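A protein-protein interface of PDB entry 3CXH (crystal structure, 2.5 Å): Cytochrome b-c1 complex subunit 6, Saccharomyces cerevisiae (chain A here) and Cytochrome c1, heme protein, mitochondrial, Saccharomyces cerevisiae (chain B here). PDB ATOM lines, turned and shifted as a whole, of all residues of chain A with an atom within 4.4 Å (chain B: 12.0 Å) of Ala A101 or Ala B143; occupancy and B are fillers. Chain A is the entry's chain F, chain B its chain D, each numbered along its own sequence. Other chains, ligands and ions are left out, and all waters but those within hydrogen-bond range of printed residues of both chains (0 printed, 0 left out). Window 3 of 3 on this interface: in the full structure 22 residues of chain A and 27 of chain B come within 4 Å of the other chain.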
ATOM      1  N   TYR A  97     -18.386   1.232 -12.928  1.00  0.00           N
ATOM      2  CA  TYR A  97     -19.252   0.123 -13.291  1.00  0.00           C
ATOM      3  C   TYR A  97     -20.620   0.662 -13.665  1.00  0.00           C
ATOM      4  O   TYR A  97     -21.118   0.409 -14.760  1.00  0.00           O
ATOM      5  CB  TYR A  97     -19.396  -0.882 -12.141  1.00  0.00           C
ATOM      6  CG  TYR A  97     -20.502  -1.888 -12.389  1.00  0.00           C
ATOM      7  CD1 TYR A  97     -20.328  -2.941 -13.288  1.00  0.00           C
ATOM      8  CD2 TYR A  97     -21.747  -1.747 -11.776  1.00  0.00           C
ATOM      9  CE1 TYR A  97     -21.371  -3.826 -13.571  1.00  0.00           C
ATOM     10  CE2 TYR A  97     -22.793  -2.622 -12.053  1.00  0.00           C
ATOM     11  CZ  TYR A  97     -22.602  -3.658 -12.950  1.00  0.00           C
ATOM     12  OH  TYR A  97     -23.642  -4.519 -13.227  1.00  0.00           O
ATOM     13  N   GLU A  98     -21.212   1.422 -12.747  1.00  0.00           N
ATOM     14  CA  GLU A  98     -22.530   2.004 -12.954  1.00  0.00           C
ATOM     15  C   GLU A  98     -22.588   2.821 -14.241  1.00  0.00           C
ATOM     16  O   GLU A  98     -23.588   2.788 -14.950  1.00  0.00           O
ATOM     17  CB  GLU A  98     -22.936   2.837 -11.743  1.00  0.00           C
ATOM     18  CG  GLU A  98     -24.415   2.738 -11.405  1.00  0.00           C
ATOM     19  CD  GLU A  98     -24.922   1.294 -11.306  1.00  0.00           C
ATOM     20  OE1 GLU A  98     -25.809   0.917 -12.109  1.00  0.00           O
ATOM     21  OE2 GLU A  98     -24.450   0.541 -10.422  1.00  0.00           O
ATOM     22  N   GLU A  99     -21.496   3.502 -14.570  1.00  0.00           N
ATOM     23  CA  GLU A  99     -21.442   4.286 -15.798  1.00  0.00           C
ATOM     24  C   GLU A  99     -21.557   3.300 -16.966  1.00  0.00           C
ATOM     25  O   GLU A  99     -22.220   3.577 -17.965  1.00  0.00           O
ATOM     26  CB  GLU A  99     -20.127   5.085 -15.887  1.00  0.00           C
ATOM     27  CG  GLU A  99     -20.132   6.205 -16.944  1.00  0.00           C
ATOM     28  CD  GLU A  99     -18.745   6.825 -17.199  1.00  0.00           C
ATOM     29  OE1 GLU A  99     -18.137   7.396 -16.256  1.00  0.00           O
ATOM     30  OE2 GLU A  99     -18.268   6.752 -18.358  1.00  0.00           O
ATOM     31  N   CYS A 100     -20.945   2.126 -16.804  1.00  0.00           N
ATOM     32  CA  CYS A 100     -20.973   1.080 -17.824  1.00  0.00           C
ATOM     33  C   CYS A 100     -22.366   0.448 -17.911  1.00  0.00           C
ATOM     34  O   CYS A 100     -22.877   0.203 -19.010  1.00  0.00           O
ATOM     35  CB  CYS A 100     -19.923   0.002 -17.512  1.00  0.00           C
ATOM     36  SG  CYS A 100     -19.847  -1.402 -18.678  1.00  0.00           S
ATOM     37  N   ALA A 101     -22.982   0.208 -16.754  1.00  0.00           N
ATOM     38  CA  ALA A 101     -24.310  -0.395 -16.696  1.00  0.00           C
ATOM     39  C   ALA A 101     -25.357   0.446 -17.419  1.00  0.00           C
ATOM     40  O   ALA A 101     -26.306  -0.096 -17.986  1.00  0.00           O
ATOM     41  CB  ALA A 101     -24.727  -0.635 -15.250  1.00  0.00           C
ATOM     42  N   GLU A 102     -25.172   1.766 -17.406  1.00  0.00           N
ATOM     43  CA  GLU A 102     -26.093   2.683 -18.064  1.00  0.00           C
ATOM     44  C   GLU A 102     -25.932   2.597 -19.567  1.00  0.00           C
ATOM     45  O   GLU A 102     -26.912   2.484 -20.299  1.00  0.00           O
ATOM     46  CB  GLU A 102     -25.843   4.128 -17.621  1.00  0.00           C
ATOM     47  CG  GLU A 102     -26.287   4.447 -16.199  1.00  0.00           C
ATOM     48  CD  GLU A 102     -26.047   5.909 -15.818  1.00  0.00           C
ATOM     49  OE1 GLU A 102     -25.068   6.515 -16.321  1.00  0.00           O
ATOM     50  OE2 GLU A 102     -26.837   6.446 -15.009  1.00  0.00           O
ATOM     51  N   ARG A 103     -24.685   2.663 -20.018  1.00  0.00           N
ATOM     52  CA  ARG A 103     -24.378   2.592 -21.437  1.00  0.00           C
ATOM     53  C   ARG A 103     -24.932   1.301 -22.032  1.00  0.00           C
ATOM     54  O   ARG A 103     -25.424   1.290 -23.161  1.00  0.00           O
ATOM     55  CB  ARG A 103     -22.867   2.683 -21.645  1.00  0.00           C
ATOM     56  CG  ARG A 103     -22.428   2.686 -23.100  1.00  0.00           C
ATOM     57  CD  ARG A 103     -20.974   3.134 -23.251  1.00  0.00           C
ATOM     58  NE  ARG A 103     -20.034   2.264 -22.548  1.00  0.00           N
ATOM     59  CZ  ARG A 103     -19.507   2.530 -21.358  1.00  0.00           C
ATOM     60  NH1 ARG A 103     -18.663   1.671 -20.807  1.00  0.00           N
ATOM     61  NH2 ARG A 103     -19.822   3.645 -20.712  1.00  0.00           N
ATOM     62  N   VAL A 104     -24.904   0.236 -21.236  1.00  0.00           N
ATOM     63  CA  VAL A 104     -25.400  -1.064 -21.669  1.00  0.00           C
ATOM     64  C   VAL A 104     -26.923  -1.127 -21.794  1.00  0.00           C
ATOM     65  O   VAL A 104     -27.430  -1.585 -22.816  1.00  0.00           O
ATOM     66  CB  VAL A 104     -24.891  -2.205 -20.747  1.00  0.00           C
ATOM     67  CG1 VAL A 104     -25.639  -3.496 -21.033  1.00  0.00           C
ATOM     68  CG2 VAL A 104     -23.401  -2.428 -20.966  1.00  0.00           C
ATOM     69  N   LYS A 105     -27.650  -0.670 -20.773  1.00  0.00           N
ATOM     70  CA  LYS A 105     -29.113  -0.704 -20.828  1.00  0.00           C
ATOM     71  C   LYS A 105     -29.631   0.153 -21.982  1.00  0.00           C
ATOM     72  O   LYS A 105     -30.632  -0.184 -22.615  1.00  0.00           O
ATOM     73  CB  LYS A 105     -29.750  -0.263 -19.501  1.00  0.00           C
ATOM     74  CG  LYS A 105     -29.870   1.245 -19.284  1.00  0.00           C
ATOM     75  CD  LYS A 105     -30.820   1.551 -18.123  1.00  0.00           C
ATOM     76  CE  LYS A 105     -30.936   3.052 -17.843  1.00  0.00           C
ATOM     77  NZ  LYS A 105     -29.661   3.665 -17.352  1.00  0.00           N
ATOM     78  N   ASP A 121     -20.464  -5.771 -22.292  1.00  0.00           N
ATOM     79  CA  ASP A 121     -20.835  -6.261 -20.969  1.00  0.00           C
ATOM     80  C   ASP A 121     -19.979  -5.487 -19.974  1.00  0.00           C
ATOM     81  O   ASP A 121     -19.009  -4.846 -20.368  1.00  0.00           O
ATOM     82  CB  ASP A 121     -20.569  -7.769 -20.854  1.00  0.00           C
ATOM     83  CG  ASP A 121     -19.101  -8.124 -21.043  1.00  0.00           C
ATOM     84  OD1 ASP A 121     -18.631  -8.152 -22.203  1.00  0.00           O
ATOM     85  OD2 ASP A 121     -18.417  -8.368 -20.027  1.00  0.00           O
ATOM     86  N   CYS A 122     -20.312  -5.550 -18.690  1.00  0.00           N
ATOM     87  CA  CYS A 122     -19.538  -4.814 -17.703  1.00  0.00           C
ATOM     88  C   CYS A 122     -18.745  -5.676 -16.737  1.00  0.00           C
ATOM     89  O   CYS A 122     -18.479  -5.262 -15.601  1.00  0.00           O
ATOM     90  CB  CYS A 122     -20.444  -3.853 -16.938  1.00  0.00           C
ATOM     91  SG  CYS A 122     -21.298  -2.681 -18.032  1.00  0.00           S
ATOM     92  N   ALA B   4     -13.426 -12.797 -17.839  1.00  0.00           N
ATOM     93  CA  ALA B   4     -14.602 -13.637 -17.632  1.00  0.00           C
ATOM     94  C   ALA B   4     -14.251 -15.124 -17.740  1.00  0.00           C
ATOM     95  O   ALA B   4     -14.643 -15.925 -16.894  1.00  0.00           O
ATOM     96  CB  ALA B   4     -15.695 -13.278 -18.638  1.00  0.00           C
ATOM     97  N   PRO B 138     -23.326 -12.666  -6.508  1.00  0.00           N
ATOM     98  CA  PRO B 138     -23.946 -11.342  -6.486  1.00  0.00           C
ATOM     99  C   PRO B 138     -25.437 -11.627  -6.543  1.00  0.00           C
ATOM    100  O   PRO B 138     -25.845 -12.785  -6.669  1.00  0.00           O
ATOM    101  CB  PRO B 138     -23.489 -10.727  -7.812  1.00  0.00           C
ATOM    102  CG  PRO B 138     -22.292 -11.520  -8.199  1.00  0.00           C
ATOM    103  CD  PRO B 138     -22.681 -12.906  -7.805  1.00  0.00           C
ATOM    104  N   ASP B 139     -26.258 -10.595  -6.456  1.00  0.00           N
ATOM    105  CA  ASP B 139     -27.698 -10.807  -6.535  1.00  0.00           C
ATOM    106  C   ASP B 139     -28.105 -10.789  -7.995  1.00  0.00           C
ATOM    107  O   ASP B 139     -29.065 -11.452  -8.400  1.00  0.00           O
ATOM    108  CB  ASP B 139     -28.440  -9.722  -5.762  1.00  0.00           C
ATOM    109  CG  ASP B 139     -28.244  -9.852  -4.270  1.00  0.00           C
ATOM    110  OD1 ASP B 139     -29.166 -10.358  -3.596  1.00  0.00           O
ATOM    111  OD2 ASP B 139     -27.154  -9.483  -3.776  1.00  0.00           O
ATOM    112  N   GLU B 140     -27.298 -10.098  -8.792  1.00  0.00           N
ATOM    113  CA  GLU B 140     -27.558  -9.951 -10.208  1.00  0.00           C
ATOM    114  C   GLU B 140     -26.236  -9.949 -10.968  1.00  0.00           C
ATOM    115  O   GLU B 140     -25.233  -9.429 -10.474  1.00  0.00           O
ATOM    116  CB  GLU B 140     -28.281  -8.615 -10.422  1.00  0.00           C
ATOM    117  CG  GLU B 140     -28.963  -8.440 -11.773  1.00  0.00           C
ATOM    118  CD  GLU B 140     -30.278  -9.206 -11.899  1.00  0.00           C
ATOM    119  OE1 GLU B 140     -30.911  -9.084 -12.973  1.00  0.00           O
ATOM    120  OE2 GLU B 140     -30.681  -9.919 -10.942  1.00  0.00           O
ATOM    121  N   PRO B 141     -26.201 -10.581 -12.157  1.00  0.00           N
ATOM    122  CA  PRO B 141     -24.981 -10.630 -12.974  1.00  0.00           C
ATOM    123  C   PRO B 141     -24.643  -9.247 -13.535  1.00  0.00           C
ATOM    124  O   PRO B 141     -25.526  -8.399 -13.697  1.00  0.00           O
ATOM    125  CB  PRO B 141     -25.365 -11.595 -14.099  1.00  0.00           C
ATOM    126  CG  PRO B 141     -26.845 -11.398 -14.223  1.00  0.00           C
ATOM    127  CD  PRO B 141     -27.274 -11.376 -12.779  1.00  0.00           C
ATOM    128  N   PRO B 142     -23.356  -8.991 -13.819  1.00  0.00           N
ATOM    129  CA  PRO B 142     -22.991  -7.680 -14.361  1.00  0.00           C
ATOM    130  C   PRO B 142     -23.767  -7.379 -15.646  1.00  0.00           C
ATOM    131  O   PRO B 142     -24.207  -8.295 -16.350  1.00  0.00           O
ATOM    132  CB  PRO B 142     -21.478  -7.807 -14.589  1.00  0.00           C
ATOM    133  CG  PRO B 142     -21.251  -9.286 -14.692  1.00  0.00           C
ATOM    134  CD  PRO B 142     -22.168  -9.840 -13.652  1.00  0.00           C
ATOM    135  N   ALA B 143     -23.975  -6.091 -15.905  1.00  0.00           N
ATOM    136  CA  ALA B 143     -24.723  -5.637 -17.071  1.00  0.00           C
ATOM    137  C   ALA B 143     -24.234  -6.210 -18.395  1.00  0.00           C
ATOM    138  O   ALA B 143     -23.030  -6.332 -18.627  1.00  0.00           O
ATOM    139  CB  ALA B 143     -24.717  -4.120 -17.126  1.00  0.00           C
ATOM    140  N   GLY B 144     -25.183  -6.585 -19.247  1.00  0.00           N
ATOM    141  CA  GLY B 144     -24.852  -7.120 -20.556  1.00  0.00           C
ATOM    142  C   GLY B 144     -24.509  -8.594 -20.611  1.00  0.00           C
ATOM    143  O   GLY B 144     -24.273  -9.127 -21.696  1.00  0.00           O
ATOM    144  N   VAL B 145     -24.465  -9.252 -19.455  1.00  0.00           N
ATOM    145  CA  VAL B 145     -24.143 -10.675 -19.396  1.00  0.00           C
ATOM    146  C   VAL B 145     -25.416 -11.518 -19.508  1.00  0.00           C
ATOM    147  O   VAL B 145     -26.306 -11.438 -18.654  1.00  0.00           O
ATOM    148  CB  VAL B 145     -23.353 -11.022 -18.097  1.00  0.00           C
ATOM    149  CG1 VAL B 145     -23.150 -12.520 -17.969  1.00  0.00           C
ATOM    150  CG2 VAL B 145     -22.002 -10.331 -18.113  1.00  0.00           C
ATOM    151  N   ALA B 146     -25.509 -12.289 -20.592  1.00  0.00           N
ATOM    152  CA  ALA B 146     -26.663 -13.152 -20.839  1.00  0.00           C
ATOM    153  C   ALA B 146     -26.508 -14.478 -20.097  1.00  0.00           C
ATOM    154  O   ALA B 146     -25.656 -15.300 -20.442  1.00  0.00           O
ATOM    155  CB  ALA B 146     -26.829 -13.399 -22.337  1.00  0.00           C
ATOM    156  N   LEU B 147     -27.336 -14.680 -19.078  1.00  0.00           N
ATOM    157  CA  LEU B 147     -27.286 -15.894 -18.274  1.00  0.00           C
ATOM    158  C   LEU B 147     -28.318 -16.916 -18.779  1.00  0.00           C
ATOM    159  O   LEU B 147     -29.527 -16.666 -18.723  1.00  0.00           O
ATOM    160  CB  LEU B 147     -27.547 -15.526 -16.808  1.00  0.00           C
ATOM    161  CG  LEU B 147     -27.015 -16.391 -15.662  1.00  0.00           C
ATOM    162  CD1 LEU B 147     -25.507 -16.535 -15.758  1.00  0.00           C
ATOM    163  CD2 LEU B 147     -27.406 -15.745 -14.332  1.00  0.00           C
ATOM    164  N   TYR B 153     -24.911 -16.407 -11.768  1.00  0.00           N
ATOM    165  CA  TYR B 153     -23.632 -15.741 -11.935  1.00  0.00           C
ATOM    166  C   TYR B 153     -22.788 -15.774 -10.673  1.00  0.00           C
ATOM    167  O   TYR B 153     -23.290 -15.575  -9.571  1.00  0.00           O
ATOM    168  CB  TYR B 153     -23.805 -14.290 -12.389  1.00  0.00           C
ATOM    169  CG  TYR B 153     -22.484 -13.606 -12.691  1.00  0.00           C
ATOM    170  CD1 TYR B 153     -21.921 -13.682 -13.962  1.00  0.00           C
ATOM    171  CD2 TYR B 153     -21.762 -12.946 -11.687  1.00  0.00           C
ATOM    172  CE1 TYR B 153     -20.676 -13.133 -14.230  1.00  0.00           C
ATOM    173  CE2 TYR B 153     -20.507 -12.396 -11.948  1.00  0.00           C
ATOM    174  CZ  TYR B 153     -19.971 -12.500 -13.225  1.00  0.00           C
ATOM    175  OH  TYR B 153     -18.712 -12.007 -13.504  1.00  0.00           O
ATOM    176  N   ASN B 154     -21.507 -16.074 -10.862  1.00  0.00           N
ATOM    177  CA  ASN B 154     -20.515 -16.089  -9.800  1.00  0.00           C
ATOM    178  C   ASN B 154     -19.211 -15.781 -10.513  1.00  0.00           C
ATOM    179  O   ASN B 154     -18.721 -16.584 -11.300  1.00  0.00           O
ATOM    180  CB  ASN B 154     -20.433 -17.436  -9.095  1.00  0.00           C
ATOM    181  CG  ASN B 154     -19.551 -17.383  -7.864  1.00  0.00           C
ATOM    182  OD1 ASN B 154     -18.407 -16.909  -7.921  1.00  0.00           O
ATOM    183  ND2 ASN B 154     -20.072 -17.859  -6.741  1.00  0.00           N
ATOM    184  N   PRO B 155     -18.602 -14.632 -10.199  1.00  0.00           N
ATOM    185  CA  PRO B 155     -17.347 -14.187 -10.813  1.00  0.00           C
ATOM    186  C   PRO B 155     -16.113 -15.069 -10.605  1.00  0.00           C
ATOM    187  O   PRO B 155     -15.222 -15.072 -11.441  1.00  0.00           O
ATOM    188  CB  PRO B 155     -17.165 -12.797 -10.213  1.00  0.00           C
ATOM    189  CG  PRO B 155     -17.682 -12.999  -8.821  1.00  0.00           C
ATOM    190  CD  PRO B 155     -18.969 -13.752  -9.075  1.00  0.00           C
ATOM    191  N   GLY B 159     -15.803 -18.520 -16.568  1.00  0.00           N
ATOM    192  CA  GLY B 159     -16.932 -18.337 -17.465  1.00  0.00           C
ATOM    193  C   GLY B 159     -18.052 -17.565 -16.776  1.00  0.00           C
ATOM    194  O   GLY B 159     -18.979 -17.070 -17.432  1.00  0.00           O
ATOM    195  N   GLY B 160     -17.977 -17.506 -15.443  1.00  0.00           N
ATOM    196  CA  GLY B 160     -18.955 -16.796 -14.633  1.00  0.00           C
ATOM    197  C   GLY B 160     -20.319 -17.439 -14.473  1.00  0.00           C
ATOM    198  O   GLY B 160     -21.075 -17.061 -13.580  1.00  0.00           O
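O of Ala B143 lies within hydrogen-bond range of N of Cys A122 (2.8 Å). N of Ala B143 lies within hydrogen-bond range of OH of Tyr A97 (3.1 Å).
Of chain B, only Ala B143 (3.8 Å) comes within 4 Å of Ala A101. Of chain B, only Pro B142 (3.4 Å) and Ala B143 (3.1 Å) come within 4 Å of Tyr A97. No residue of chain B comes within 4 Å of Glu A98. No residue of chain B comes within 4 Å of Cys A100. No residue of chain B comes within 4 Å of Glu A102. No residue of chain B comes within 4 Å of Arg A103. Of chain B, only Gly B144 (3.6 Å) comes within 4 Å of Val A104. Lys A105 touches none of the printed residues of chain B. Of chain B, only Ala B143 (2.8 Å) comes within 4 Å of Cys A122. Of the printed residues of chain A, Pro B142 touches Tyr A97. Of the printed residues of chain A, Gly B144 touches Val A104 (3.6 Å). Val B145 touches none of the printed residues of chain A. The nearest residue of chain B that does not touch Ala A101 is Gly B144 (6.7 Å). The nearest printed residue of chain A that does not touch Pro B142 is Cys A122 (4.1 Å).
Among the printed residues, merely in contact across the chains: Asp A121 with Ala B143 (3.2 Å), Tyr A97 with Pro B142 (3.4 Å), Val A104 with Gly B144 (3.6 Å) and Ala A101 with Ala B143 (3.8 Å).
The side-chain sulfur (SG) of Cys A122 lies within hydrogen-bond range of the backbone NH (N) of Ala A101 (3.6 Å). SG of Cys A100 forms a disulfide with SG of Cys A122 (2.0 Å).
Of the 16 printed residues of chain B, 3 touch a printed residue of chain A. Printed residues of chain B that touch a printed residue of chain A: Pro B142, Ala B143 and Gly B144. Hydrophobic or aromatic side chains of chain B within 4 Å of the printed part of chain A: Ala B143. Hydrophobic or aromatic side chains of chain A within 4 Å of the printed part of chain B: Tyr A97, Ala A101 and Val A104. Among the printed residues, 6 pairs touch across the chains. Among the printed residues, no Asp or Glu carboxylate lies within 4 Å of a Lys or Arg side-chain nitrogen of the other chain.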
